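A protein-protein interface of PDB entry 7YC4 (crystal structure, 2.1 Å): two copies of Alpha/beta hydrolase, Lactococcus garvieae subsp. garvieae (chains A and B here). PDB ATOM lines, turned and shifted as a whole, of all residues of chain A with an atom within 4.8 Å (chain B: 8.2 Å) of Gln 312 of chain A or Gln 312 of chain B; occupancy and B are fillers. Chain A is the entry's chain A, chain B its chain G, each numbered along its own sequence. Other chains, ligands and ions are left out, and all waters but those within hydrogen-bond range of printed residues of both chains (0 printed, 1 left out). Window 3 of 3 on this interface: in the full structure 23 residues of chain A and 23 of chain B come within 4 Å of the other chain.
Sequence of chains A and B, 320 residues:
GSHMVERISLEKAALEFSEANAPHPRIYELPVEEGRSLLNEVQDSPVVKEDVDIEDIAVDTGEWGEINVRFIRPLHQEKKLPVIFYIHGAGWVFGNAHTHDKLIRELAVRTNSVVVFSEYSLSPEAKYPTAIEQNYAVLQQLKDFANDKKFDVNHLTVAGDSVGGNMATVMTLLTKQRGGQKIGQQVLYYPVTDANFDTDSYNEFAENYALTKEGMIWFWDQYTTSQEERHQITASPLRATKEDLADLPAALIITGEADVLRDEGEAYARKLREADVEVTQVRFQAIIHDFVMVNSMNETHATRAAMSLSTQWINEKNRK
OE1 of Gln 312 of chain B lies close to NE2 of Gln 312 of chain A (3.3 Å).
The side-chain carboxylate of Glu 316 of chain A is in salt-bridge range of the guanidinium group of Arg 110 of chain B (3.7 Å).
The backbone NH of Leu 309 of chain A sits close to the side-chain amide nitrogen of Gln 312 of chain B (3.4 Å).
The side-chain amide nitrogen of Gln 312 of chain B sits close to the backbone carbonyl oxygen of Ser 308 of chain A.
OE1 of Gln 312 of chain B sits close to O of Ser 308 of chain B.
The backbone carbonyl oxygen (O) of Ser 308 of chain A is in hydrogen-bond range of the side-chain hydroxyl (OG1) of Thr 311 of chain A, 3.2 Å away.
The guanidinium group (NH2) of Arg 110 of chain B sits at hydrogen-bond distance from the side-chain hydroxyl (OG) of Ser 308 of chain B (2.9 Å).
O of Arg 304 of chain B lies within hydrogen-bond range of OG of Ser 308 of chain B, at 3.3 Å.
The backbone carbonyl oxygen of Arg 110 of chain B lies within hydrogen-bond range of the side-chain amide nitrogen of Asn 315 of chain B (3.1 Å).
The side-chain hydroxyl of Thr 311 of chain B is in hydrogen-bond range of the backbone carbonyl oxygen of Ser 308 of chain B (3.4 Å).
Among the printed residues, merely in contact across the chains: Leu 309 of chain A with Ala 305 of chain B (3.6 Å) and Glu 316 of chain A with Ser 308 of chain B (3.7 Å).
Gln 312 of chain A touches just one residue of chain B: Gln 312.
Of chain A, only Ser 308 (3.2 Å), Leu 309 (3.4 Å) and Gln 312 (2.8 Å) come within 4 Å of Gln 312 of chain B.
Printed residues of chain A within 4 Å of Ala 305 of chain B: Leu 309 (3.6 Å).
Printed residues of chain A within 4 Å of Ser 308 of chain B: Glu 316 (3.7 Å).
Printed residues of chain B within 4 Å of Glu 316 of chain A: Arg 110 and Ser 308.
Printed residues of chain A within 4 Å of Arg 110 of chain B: Glu 316 (3.7 Å).
Of the printed residues of chain B, Leu 309 of chain A touches Ala 305 (3.6 Å) and Gln 312 (3.4 Å).
Thr 311 of chain B touches none of the printed residues of chain A.
Asn 315 of chain B touches none of the printed residues of chain A.
The nearest residue of chain B that does not touch Gln 312 of chain A is Arg 110 of chain B (5.0 Å).
The nearest printed residue of chain A that does not touch Arg 110 of chain B is Gln 312 of chain A (5.0 Å).
Printed residues of chain A that touch a printed residue of chain B: Ser 308, Leu 309, Gln 312 and Glu 316.
Ser 308 of chain A touches Gln 312 of chain B, but with the chains exchanged Gln 312 of chain A does not touch Ser 308 of chain B (5.0 Å).
Leu 309 of chain A touches Gln 312 of chain B, but with the chains exchanged Gln 312 of chain A does not touch Leu 309 of chain B (6.9 Å).
Gln 312 of chain B touches its own counterpart, Gln 312 of chain A.
Glu 316 of chain A touches Ser 308 of chain B, but with the chains exchanged Ser 308 of chain A does not touch Glu 316 of chain B (6.5 Å).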
ATOM      1  N   SER A 308     -27.696 -15.985 -20.291  1.00  0.00           N
ATOM      2  CA  SER A 308     -27.279 -15.415 -21.592  1.00  0.00           C
ATOM      3  C   SER A 308     -27.538 -16.437 -22.711  1.00  0.00           C
ATOM      4  O   SER A 308     -28.173 -16.038 -23.708  1.00  0.00           O
ATOM      5  CB  SER A 308     -25.881 -14.922 -21.541  1.00  0.00           C
ATOM      6  OG  SER A 308     -25.882 -13.703 -20.786  1.00  0.00           O
ATOM      7  N   LEU A 309     -27.167 -17.702 -22.524  1.00  0.00           N
ATOM      8  CA  LEU A 309     -27.431 -18.754 -23.538  1.00  0.00           C
ATOM      9  C   LEU A 309     -28.937 -18.949 -23.738  1.00  0.00           C
ATOM     10  O   LEU A 309     -29.360 -18.954 -24.898  1.00  0.00           O
ATOM     11  CB  LEU A 309     -26.758 -20.065 -23.131  1.00  0.00           C
ATOM     12  CG  LEU A 309     -26.862 -21.171 -24.179  1.00  0.00           C
ATOM     13  CD1 LEU A 309     -25.898 -20.904 -25.324  1.00  0.00           C
ATOM     14  CD2 LEU A 309     -26.632 -22.528 -23.564  1.00  0.00           C
ATOM     15  N   SER A 310     -29.739 -19.048 -22.666  1.00  0.00           N
ATOM     16  CA  SER A 310     -31.190 -19.338 -22.775  1.00  0.00           C
ATOM     17  C   SER A 310     -31.913 -18.150 -23.431  1.00  0.00           C
ATOM     18  O   SER A 310     -32.754 -18.372 -24.321  1.00  0.00           O
ATOM     19  CB  SER A 310     -31.795 -19.731 -21.442  1.00  0.00           C
ATOM     20  OG  SER A 310     -31.568 -18.741 -20.446  1.00  0.00           O
ATOM     21  N   THR A 311     -31.577 -16.914 -23.068  1.00  0.00           N
ATOM     22  CA  THR A 311     -32.287 -15.716 -23.578  1.00  0.00           C
ATOM     23  C   THR A 311     -31.981 -15.527 -25.081  1.00  0.00           C
ATOM     24  O   THR A 311     -32.928 -15.171 -25.873  1.00  0.00           O
ATOM     25  CB  THR A 311     -32.023 -14.501 -22.676  1.00  0.00           C
ATOM     26  OG1 THR A 311     -30.628 -14.235 -22.591  1.00  0.00           O
ATOM     27  CG2 THR A 311     -32.568 -14.712 -21.281  1.00  0.00           C
ATOM     28  N   GLN A 312     -30.737 -15.724 -25.476  1.00  0.00           N
ATOM     29  CA  GLN A 312     -30.294 -15.594 -26.893  1.00  0.00           C
ATOM     30  C   GLN A 312     -30.926 -16.711 -27.724  1.00  0.00           C
ATOM     31  O   GLN A 312     -31.392 -16.427 -28.869  1.00  0.00           O
ATOM     32  CB  GLN A 312     -28.776 -15.694 -27.033  1.00  0.00           C
ATOM     33  CG  GLN A 312     -28.069 -14.456 -26.530  1.00  0.00           C
ATOM     34  CD  GLN A 312     -27.799 -13.464 -27.638  1.00  0.00           C
ATOM     35  OE1 GLN A 312     -28.266 -12.328 -27.592  1.00  0.00           O
ATOM     36  NE2 GLN A 312     -27.041 -13.897 -28.635  1.00  0.00           N
ATOM     37  N   TRP A 313     -30.902 -17.930 -27.188  1.00  0.00           N
ATOM     38  CA  TRP A 313     -31.511 -19.100 -27.866  1.00  0.00           C
ATOM     39  C   TRP A 313     -32.995 -18.809 -28.145  1.00  0.00           C
ATOM     40  O   TRP A 313     -33.415 -18.986 -29.307  1.00  0.00           O
ATOM     41  CB  TRP A 313     -31.273 -20.359 -27.040  1.00  0.00           C
ATOM     42  CG  TRP A 313     -31.668 -21.634 -27.706  1.00  0.00           C
ATOM     43  CD1 TRP A 313     -30.883 -22.444 -28.469  1.00  0.00           C
ATOM     44  CD2 TRP A 313     -32.949 -22.269 -27.621  1.00  0.00           C
ATOM     45  NE1 TRP A 313     -31.591 -23.539 -28.874  1.00  0.00           N
ATOM     46  CE2 TRP A 313     -32.861 -23.463 -28.369  1.00  0.00           C
ATOM     47  CE3 TRP A 313     -34.156 -21.955 -26.986  1.00  0.00           C
ATOM     48  CZ2 TRP A 313     -33.936 -24.346 -28.483  1.00  0.00           C
ATOM     49  CZ3 TRP A 313     -35.211 -22.829 -27.100  1.00  0.00           C
ATOM     50  CH2 TRP A 313     -35.095 -24.020 -27.815  1.00  0.00           C
ATOM     51  N   ILE A 314     -33.749 -18.339 -27.147  1.00  0.00           N
ATOM     52  CA  ILE A 314     -35.173 -17.918 -27.314  1.00  0.00           C
ATOM     53  C   ILE A 314     -35.306 -16.810 -28.381  1.00  0.00           C
ATOM     54  O   ILE A 314     -36.175 -16.951 -29.254  1.00  0.00           O
ATOM     55  CB  ILE A 314     -35.788 -17.475 -25.983  1.00  0.00           C
ATOM     56  CG1 ILE A 314     -35.915 -18.651 -25.010  1.00  0.00           C
ATOM     57  CG2 ILE A 314     -37.117 -16.787 -26.209  1.00  0.00           C
ATOM     58  CD1 ILE A 314     -36.361 -18.224 -23.646  1.00  0.00           C
ATOM     59  N   ASN A 315     -34.535 -15.724 -28.295  1.00  0.00           N
ATOM     60  CA  ASN A 315     -34.548 -14.625 -29.304  1.00  0.00           C
ATOM     61  C   ASN A 315     -34.273 -15.160 -30.720  1.00  0.00           C
ATOM     62  O   ASN A 315     -34.997 -14.735 -31.633  1.00  0.00           O
ATOM     63  CB  ASN A 315     -33.568 -13.514 -28.952  1.00  0.00           C
ATOM     64  CG  ASN A 315     -33.904 -12.867 -27.632  1.00  0.00           C
ATOM     65  OD1 ASN A 315     -35.012 -13.002 -27.129  1.00  0.00           O
ATOM     66  ND2 ASN A 315     -32.949 -12.177 -27.050  1.00  0.00           N
ATOM     67  N   GLU A 316     -33.265 -16.014 -30.907  1.00  0.00           N
ATOM     68  CA  GLU A 316     -32.866 -16.608 -32.222  1.00  0.00           C
ATOM     69  C   GLU A 316     -34.024 -17.484 -32.741  1.00  0.00           C
ATOM     70  O   GLU A 316     -34.372 -17.348 -33.924  1.00  0.00           O
ATOM     71  CB  GLU A 316     -31.506 -17.323 -32.112  1.00  0.00           C
ATOM     72  CG  GLU A 316     -30.293 -16.366 -32.178  1.00  0.00           C
ATOM     73  CD  GLU A 316     -28.935 -16.808 -31.604  1.00  0.00           C
ATOM     74  OE1 GLU A 316     -27.928 -16.063 -31.779  1.00  0.00           O
ATOM     75  OE2 GLU A 316     -28.861 -17.879 -30.964  1.00  0.00           O
ATOM     76  N   LEU B 107     -15.760 -15.454 -35.206  1.00  0.00           N
ATOM     77  CA  LEU B 107     -15.318 -14.760 -33.963  1.00  0.00           C
ATOM     78  C   LEU B 107     -15.240 -13.262 -34.224  1.00  0.00           C
ATOM     79  O   LEU B 107     -15.747 -12.504 -33.386  1.00  0.00           O
ATOM     80  CB  LEU B 107     -13.958 -15.251 -33.458  1.00  0.00           C
ATOM     81  CG  LEU B 107     -13.993 -16.426 -32.485  1.00  0.00           C
ATOM     82  CD1 LEU B 107     -12.595 -16.983 -32.264  1.00  0.00           C
ATOM     83  CD2 LEU B 107     -14.642 -16.031 -31.163  1.00  0.00           C
ATOM     84  N   ARG B 110     -18.803 -11.642 -34.895  1.00  0.00           N
ATOM     85  CA  ARG B 110     -19.854 -11.699 -33.833  1.00  0.00           C
ATOM     86  C   ARG B 110     -19.356 -10.955 -32.586  1.00  0.00           C
ATOM     87  O   ARG B 110     -20.190 -10.511 -31.827  1.00  0.00           O
ATOM     88  CB  ARG B 110     -20.329 -13.137 -33.598  1.00  0.00           C
ATOM     89  CG  ARG B 110     -21.071 -13.699 -34.800  1.00  0.00           C
ATOM     90  CD  ARG B 110     -21.621 -15.099 -34.583  1.00  0.00           C
ATOM     91  NE  ARG B 110     -22.657 -15.051 -33.567  1.00  0.00           N
ATOM     92  CZ  ARG B 110     -23.246 -16.112 -33.029  1.00  0.00           C
ATOM     93  NH1 ARG B 110     -22.880 -17.321 -33.411  1.00  0.00           N
ATOM     94  NH2 ARG B 110     -24.270 -15.962 -32.188  1.00  0.00           N
ATOM     95  N   THR B 111     -18.044 -10.769 -32.420  1.00  0.00           N
ATOM     96  CA  THR B 111     -17.460 -10.003 -31.288  1.00  0.00           C
ATOM     97  C   THR B 111     -17.096  -8.593 -31.773  1.00  0.00           C
ATOM     98  O   THR B 111     -16.657  -7.808 -30.959  1.00  0.00           O
ATOM     99  CB  THR B 111     -16.260 -10.726 -30.641  1.00  0.00           C
ATOM    100  OG1 THR B 111     -15.122 -10.784 -31.519  1.00  0.00           O
ATOM    101  CG2 THR B 111     -16.618 -12.117 -30.163  1.00  0.00           C
ATOM    102  N   LEU B 252     -13.091 -18.751 -20.008  1.00  0.00           N
ATOM    103  CA  LEU B 252     -14.183 -19.557 -20.569  1.00  0.00           C
ATOM    104  C   LEU B 252     -13.576 -20.849 -21.109  1.00  0.00           C
ATOM    105  O   LEU B 252     -12.684 -20.787 -21.976  1.00  0.00           O
ATOM    106  CB  LEU B 252     -14.941 -18.792 -21.662  1.00  0.00           C
ATOM    107  CG  LEU B 252     -16.077 -19.584 -22.320  1.00  0.00           C
ATOM    108  CD1 LEU B 252     -17.062 -20.087 -21.284  1.00  0.00           C
ATOM    109  CD2 LEU B 252     -16.812 -18.752 -23.359  1.00  0.00           C
ATOM    110  N   ARG B 304     -23.421 -24.152 -32.678  1.00  0.00           N
ATOM    111  CA  ARG B 304     -24.238 -22.913 -32.617  1.00  0.00           C
ATOM    112  C   ARG B 304     -24.228 -22.396 -31.175  1.00  0.00           C
ATOM    113  O   ARG B 304     -23.953 -21.191 -30.981  1.00  0.00           O
ATOM    114  CB  ARG B 304     -25.640 -23.124 -33.195  1.00  0.00           C
ATOM    115  CG  ARG B 304     -25.640 -23.400 -34.692  1.00  0.00           C
ATOM    116  CD  ARG B 304     -25.038 -22.303 -35.573  1.00  0.00           C
ATOM    117  NE  ARG B 304     -23.614 -22.487 -35.899  1.00  0.00           N
ATOM    118  CZ  ARG B 304     -22.655 -21.590 -35.741  1.00  0.00           C
ATOM    119  NH1 ARG B 304     -21.416 -21.843 -36.149  1.00  0.00           N
ATOM    120  NH2 ARG B 304     -22.936 -20.406 -35.234  1.00  0.00           N
ATOM    121  N   ALA B 305     -24.451 -23.260 -30.187  1.00  0.00           N
ATOM    122  CA  ALA B 305     -24.573 -22.836 -28.772  1.00  0.00           C
ATOM    123  C   ALA B 305     -23.186 -22.405 -28.266  1.00  0.00           C
ATOM    124  O   ALA B 305     -23.087 -21.399 -27.547  1.00  0.00           O
ATOM    125  CB  ALA B 305     -25.240 -23.936 -27.961  1.00  0.00           C
ATOM    126  N   ALA B 306     -22.111 -23.081 -28.658  1.00  0.00           N
ATOM    127  CA  ALA B 306     -20.740 -22.767 -28.180  1.00  0.00           C
ATOM    128  C   ALA B 306     -20.271 -21.432 -28.775  1.00  0.00           C
ATOM    129  O   ALA B 306     -19.581 -20.647 -28.089  1.00  0.00           O
ATOM    130  CB  ALA B 306     -19.784 -23.878 -28.509  1.00  0.00           C
ATOM    131  N   MET B 307     -20.625 -21.183 -30.023  1.00  0.00           N
ATOM    132  CA  MET B 307     -20.277 -19.928 -30.711  1.00  0.00           C
ATOM    133  C   MET B 307     -21.078 -18.789 -30.066  1.00  0.00           C
ATOM    134  O   MET B 307     -20.470 -17.793 -29.767  1.00  0.00           O
ATOM    135  CB  MET B 307     -20.546 -20.043 -32.212  1.00  0.00           C
ATOM    136  CG  MET B 307     -19.546 -20.950 -32.930  1.00  0.00           C
ATOM    137  SD  MET B 307     -17.772 -20.705 -32.501  1.00  0.00           S
ATOM    138  CE  MET B 307     -17.575 -18.965 -32.893  1.00  0.00           C
ATOM    139  N   SER B 308     -22.369 -18.981 -29.792  1.00  0.00           N
ATOM    140  CA  SER B 308     -23.221 -17.963 -29.127  1.00  0.00           C
ATOM    141  C   SER B 308     -22.715 -17.669 -27.714  1.00  0.00           C
ATOM    142  O   SER B 308     -22.716 -16.470 -27.362  1.00  0.00           O
ATOM    143  CB  SER B 308     -24.686 -18.314 -29.140  1.00  0.00           C
ATOM    144  OG  SER B 308     -25.174 -18.143 -30.473  1.00  0.00           O
ATOM    145  N   LEU B 309     -22.403 -18.700 -26.924  1.00  0.00           N
ATOM    146  CA  LEU B 309     -21.934 -18.531 -25.522  1.00  0.00           C
ATOM    147  C   LEU B 309     -20.576 -17.809 -25.505  1.00  0.00           C
ATOM    148  O   LEU B 309     -20.404 -16.915 -24.685  1.00  0.00           O
ATOM    149  CB  LEU B 309     -21.826 -19.889 -24.817  1.00  0.00           C
ATOM    150  CG  LEU B 309     -21.013 -19.855 -23.523  1.00  0.00           C
ATOM    151  CD1 LEU B 309     -21.789 -19.129 -22.450  1.00  0.00           C
ATOM    152  CD2 LEU B 309     -20.594 -21.244 -23.062  1.00  0.00           C
ATOM    153  N   SER B 310     -19.635 -18.213 -26.356  1.00  0.00           N
ATOM    154  CA  SER B 310     -18.260 -17.685 -26.372  1.00  0.00           C
ATOM    155  C   SER B 310     -18.279 -16.239 -26.865  1.00  0.00           C
ATOM    156  O   SER B 310     -17.673 -15.404 -26.200  1.00  0.00           O
ATOM    157  CB  SER B 310     -17.342 -18.597 -27.168  1.00  0.00           C
ATOM    158  OG  SER B 310     -17.787 -18.770 -28.500  1.00  0.00           O
ATOM    159  N   THR B 311     -19.042 -15.924 -27.907  1.00  0.00           N
ATOM    160  CA  THR B 311     -19.135 -14.543 -28.442  1.00  0.00           C
ATOM    161  C   THR B 311     -19.878 -13.655 -27.433  1.00  0.00           C
ATOM    162  O   THR B 311     -19.433 -12.537 -27.292  1.00  0.00           O
ATOM    163  CB  THR B 311     -19.719 -14.493 -29.863  1.00  0.00           C
ATOM    164  OG1 THR B 311     -21.047 -14.992 -29.873  1.00  0.00           O
ATOM    165  CG2 THR B 311     -18.932 -15.299 -30.869  1.00  0.00           C
ATOM    166  N   GLN B 312     -20.942 -14.133 -26.773  1.00  0.00           N
ATOM    167  CA  GLN B 312     -21.695 -13.356 -25.746  1.00  0.00           C
ATOM    168  C   GLN B 312     -20.751 -13.066 -24.570  1.00  0.00           C
ATOM    169  O   GLN B 312     -20.728 -11.933 -24.084  1.00  0.00           O
ATOM    170  CB  GLN B 312     -22.889 -14.117 -25.152  1.00  0.00           C
ATOM    171  CG  GLN B 312     -24.103 -14.304 -26.063  1.00  0.00           C
ATOM    172  CD  GLN B 312     -24.973 -15.506 -25.713  1.00  0.00           C
ATOM    173  OE1 GLN B 312     -25.710 -16.013 -26.553  1.00  0.00           O
ATOM    174  NE2 GLN B 312     -24.885 -16.021 -24.490  1.00  0.00           N
ATOM    175  N   TRP B 313     -20.012 -14.083 -24.128  1.00  0.00           N
ATOM    176  CA  TRP B 313     -19.078 -13.972 -22.984  1.00  0.00           C
ATOM    177  C   TRP B 313     -17.974 -12.958 -23.327  1.00  0.00           C
ATOM    178  O   TRP B 313     -17.737 -12.090 -22.498  1.00  0.00           O
ATOM    179  CB  TRP B 313     -18.539 -15.341 -22.643  1.00  0.00           C
ATOM    180  CG  TRP B 313     -17.752 -15.431 -21.381  1.00  0.00           C
ATOM    181  CD1 TRP B 313     -18.232 -15.778 -20.153  1.00  0.00           C
ATOM    182  CD2 TRP B 313     -16.332 -15.253 -21.226  1.00  0.00           C
ATOM    183  NE1 TRP B 313     -17.203 -15.832 -19.248  1.00  0.00           N
ATOM    184  CE2 TRP B 313     -16.031 -15.524 -19.871  1.00  0.00           C
ATOM    185  CE3 TRP B 313     -15.289 -14.944 -22.095  1.00  0.00           C
ATOM    186  CZ2 TRP B 313     -14.735 -15.488 -19.363  1.00  0.00           C
ATOM    187  CZ3 TRP B 313     -14.004 -14.926 -21.596  1.00  0.00           C
ATOM    188  CH2 TRP B 313     -13.735 -15.170 -20.248  1.00  0.00           C
ATOM    189  N   ILE B 314     -17.344 -13.058 -24.499  1.00  0.00           N
ATOM    190  CA  ILE B 314     -16.333 -12.048 -24.966  1.00  0.00           C
ATOM    191  C   ILE B 314     -16.982 -10.648 -25.080  1.00  0.00           C
ATOM    192  O   ILE B 314     -16.344  -9.687 -24.630  1.00  0.00           O
ATOM    193  CB  ILE B 314     -15.672 -12.498 -26.275  1.00  0.00           C
ATOM    194  CG1 ILE B 314     -14.738 -13.695 -26.040  1.00  0.00           C
ATOM    195  CG2 ILE B 314     -14.940 -11.348 -26.958  1.00  0.00           C
ATOM    196  CD1 ILE B 314     -14.398 -14.447 -27.323  1.00  0.00           C
ATOM    197  N   ASN B 315     -18.158 -10.513 -25.696  1.00  0.00           N
ATOM    198  CA  ASN B 315     -18.868  -9.212 -25.849  1.00  0.00           C
ATOM    199  C   ASN B 315     -19.089  -8.568 -24.471  1.00  0.00           C
ATOM    200  O   ASN B 315     -18.833  -7.337 -24.325  1.00  0.00           O
ATOM    201  CB  ASN B 315     -20.183  -9.369 -26.610  1.00  0.00           C
ATOM    202  CG  ASN B 315     -19.911  -9.509 -28.089  1.00  0.00           C
ATOM    203  OD1 ASN B 315     -18.800  -9.251 -28.512  1.00  0.00           O
ATOM    204  ND2 ASN B 315     -20.859 -10.000 -28.864  1.00  0.00           N
ATOM    205  N   GLU B 316     -19.507  -9.365 -23.498  1.00  0.00           N
ATOM    206  CA  GLU B 316     -19.793  -8.897 -22.117  1.00  0.00           C
ATOM    207  C   GLU B 316     -18.501  -8.308 -21.548  1.00  0.00           C
ATOM    208  O   GLU B 316     -18.576  -7.247 -20.930  1.00  0.00           O
ATOM    209  CB  GLU B 316     -20.328 -10.045 -21.264  1.00  0.00           C
ATOM    210  CG  GLU B 316     -20.894  -9.619 -19.919  1.00  0.00           C
ATOM    211  CD  GLU B 316     -19.891  -9.235 -18.844  1.00  0.00           C
ATOM    212  OE1 GLU B 316     -18.821  -9.874 -18.772  1.00  0.00           O
ATOM    213  OE2 GLU B 316     -20.198  -8.295 -18.065  1.00  0.00           O
ATOM    214  N   LYS B 317     -17.372  -8.983 -21.765  1.00  0.00           N
ATOM    215  CA  LYS B 317     -16.047  -8.598 -21.222  1.00  0.00           C
ATOM    216  C   LYS B 317     -15.589  -7.288 -21.861  1.00  0.00           C
ATOM    217  O   LYS B 317     -14.922  -6.502 -21.166  1.00  0.00           O
ATOM    218  CB  LYS B 317     -15.005  -9.683 -21.507  1.00  0.00           C
ATOM    219  CG  LYS B 317     -15.148 -10.950 -20.690  1.00  0.00           C
ATOM    220  CD  LYS B 317     -14.830 -10.772 -19.231  1.00  0.00           C
ATOM    221  CE  LYS B 317     -15.520 -11.788 -18.365  1.00  0.00           C
ATOM    222  NZ  LYS B 317     -14.850 -11.875 -17.059  1.00  0.00           N
ATOM    223  N   ASN B 318     -15.895  -7.110 -23.151  1.00  0.00           N
ATOM    224  CA  ASN B 318     -15.469  -5.944 -23.973  1.00  0.00           C
ATOM    225  C   ASN B 318     -16.384  -4.738 -23.729  1.00  0.00           C
ATOM    226  O   ASN B 318     -15.891  -3.616 -23.942  1.00  0.00           O
ATOM    227  CB  ASN B 318     -15.483  -6.255 -25.468  1.00  0.00           C
ATOM    228  CG  ASN B 318     -14.327  -7.127 -25.900  1.00  0.00           C
ATOM    229  OD1 ASN B 318     -13.261  -7.090 -25.305  1.00  0.00           O
ATOM    230  ND2 ASN B 318     -14.531  -7.908 -26.948  1.00  0.00           N
ATOM    231  N   ARG B 319     -17.646  -4.950 -23.318  1.00  0.00           N
ATOM    232  CA  ARG B 319     -18.637  -3.867 -23.044  1.00  0.00           C
ATOM    233  C   ARG B 319     -18.052  -2.911 -21.996  1.00  0.00           C
ATOM    234  O   ARG B 319     -18.357  -1.691 -22.060  1.00  0.00           O
ATOM    235  CB  ARG B 319     -19.968  -4.447 -22.558  1.00  0.00           C
ATOM    236  CG  ARG B 319     -20.908  -4.858 -23.685  1.00  0.00           C
ATOM    237  CD  ARG B 319     -22.076  -5.720 -23.225  1.00  0.00           C
ATOM    238  NE  ARG B 319     -22.830  -5.108 -22.132  1.00  0.00           N
ATOM    239  CZ  ARG B 319     -22.639  -5.324 -20.827  1.00  0.00           C
ATOM    240  NH1 ARG B 319     -21.704  -6.160 -20.401  1.00  0.00           N
ATOM    241  NH2 ARG B 319     -23.396  -4.693 -19.944  1.00  0.00           N
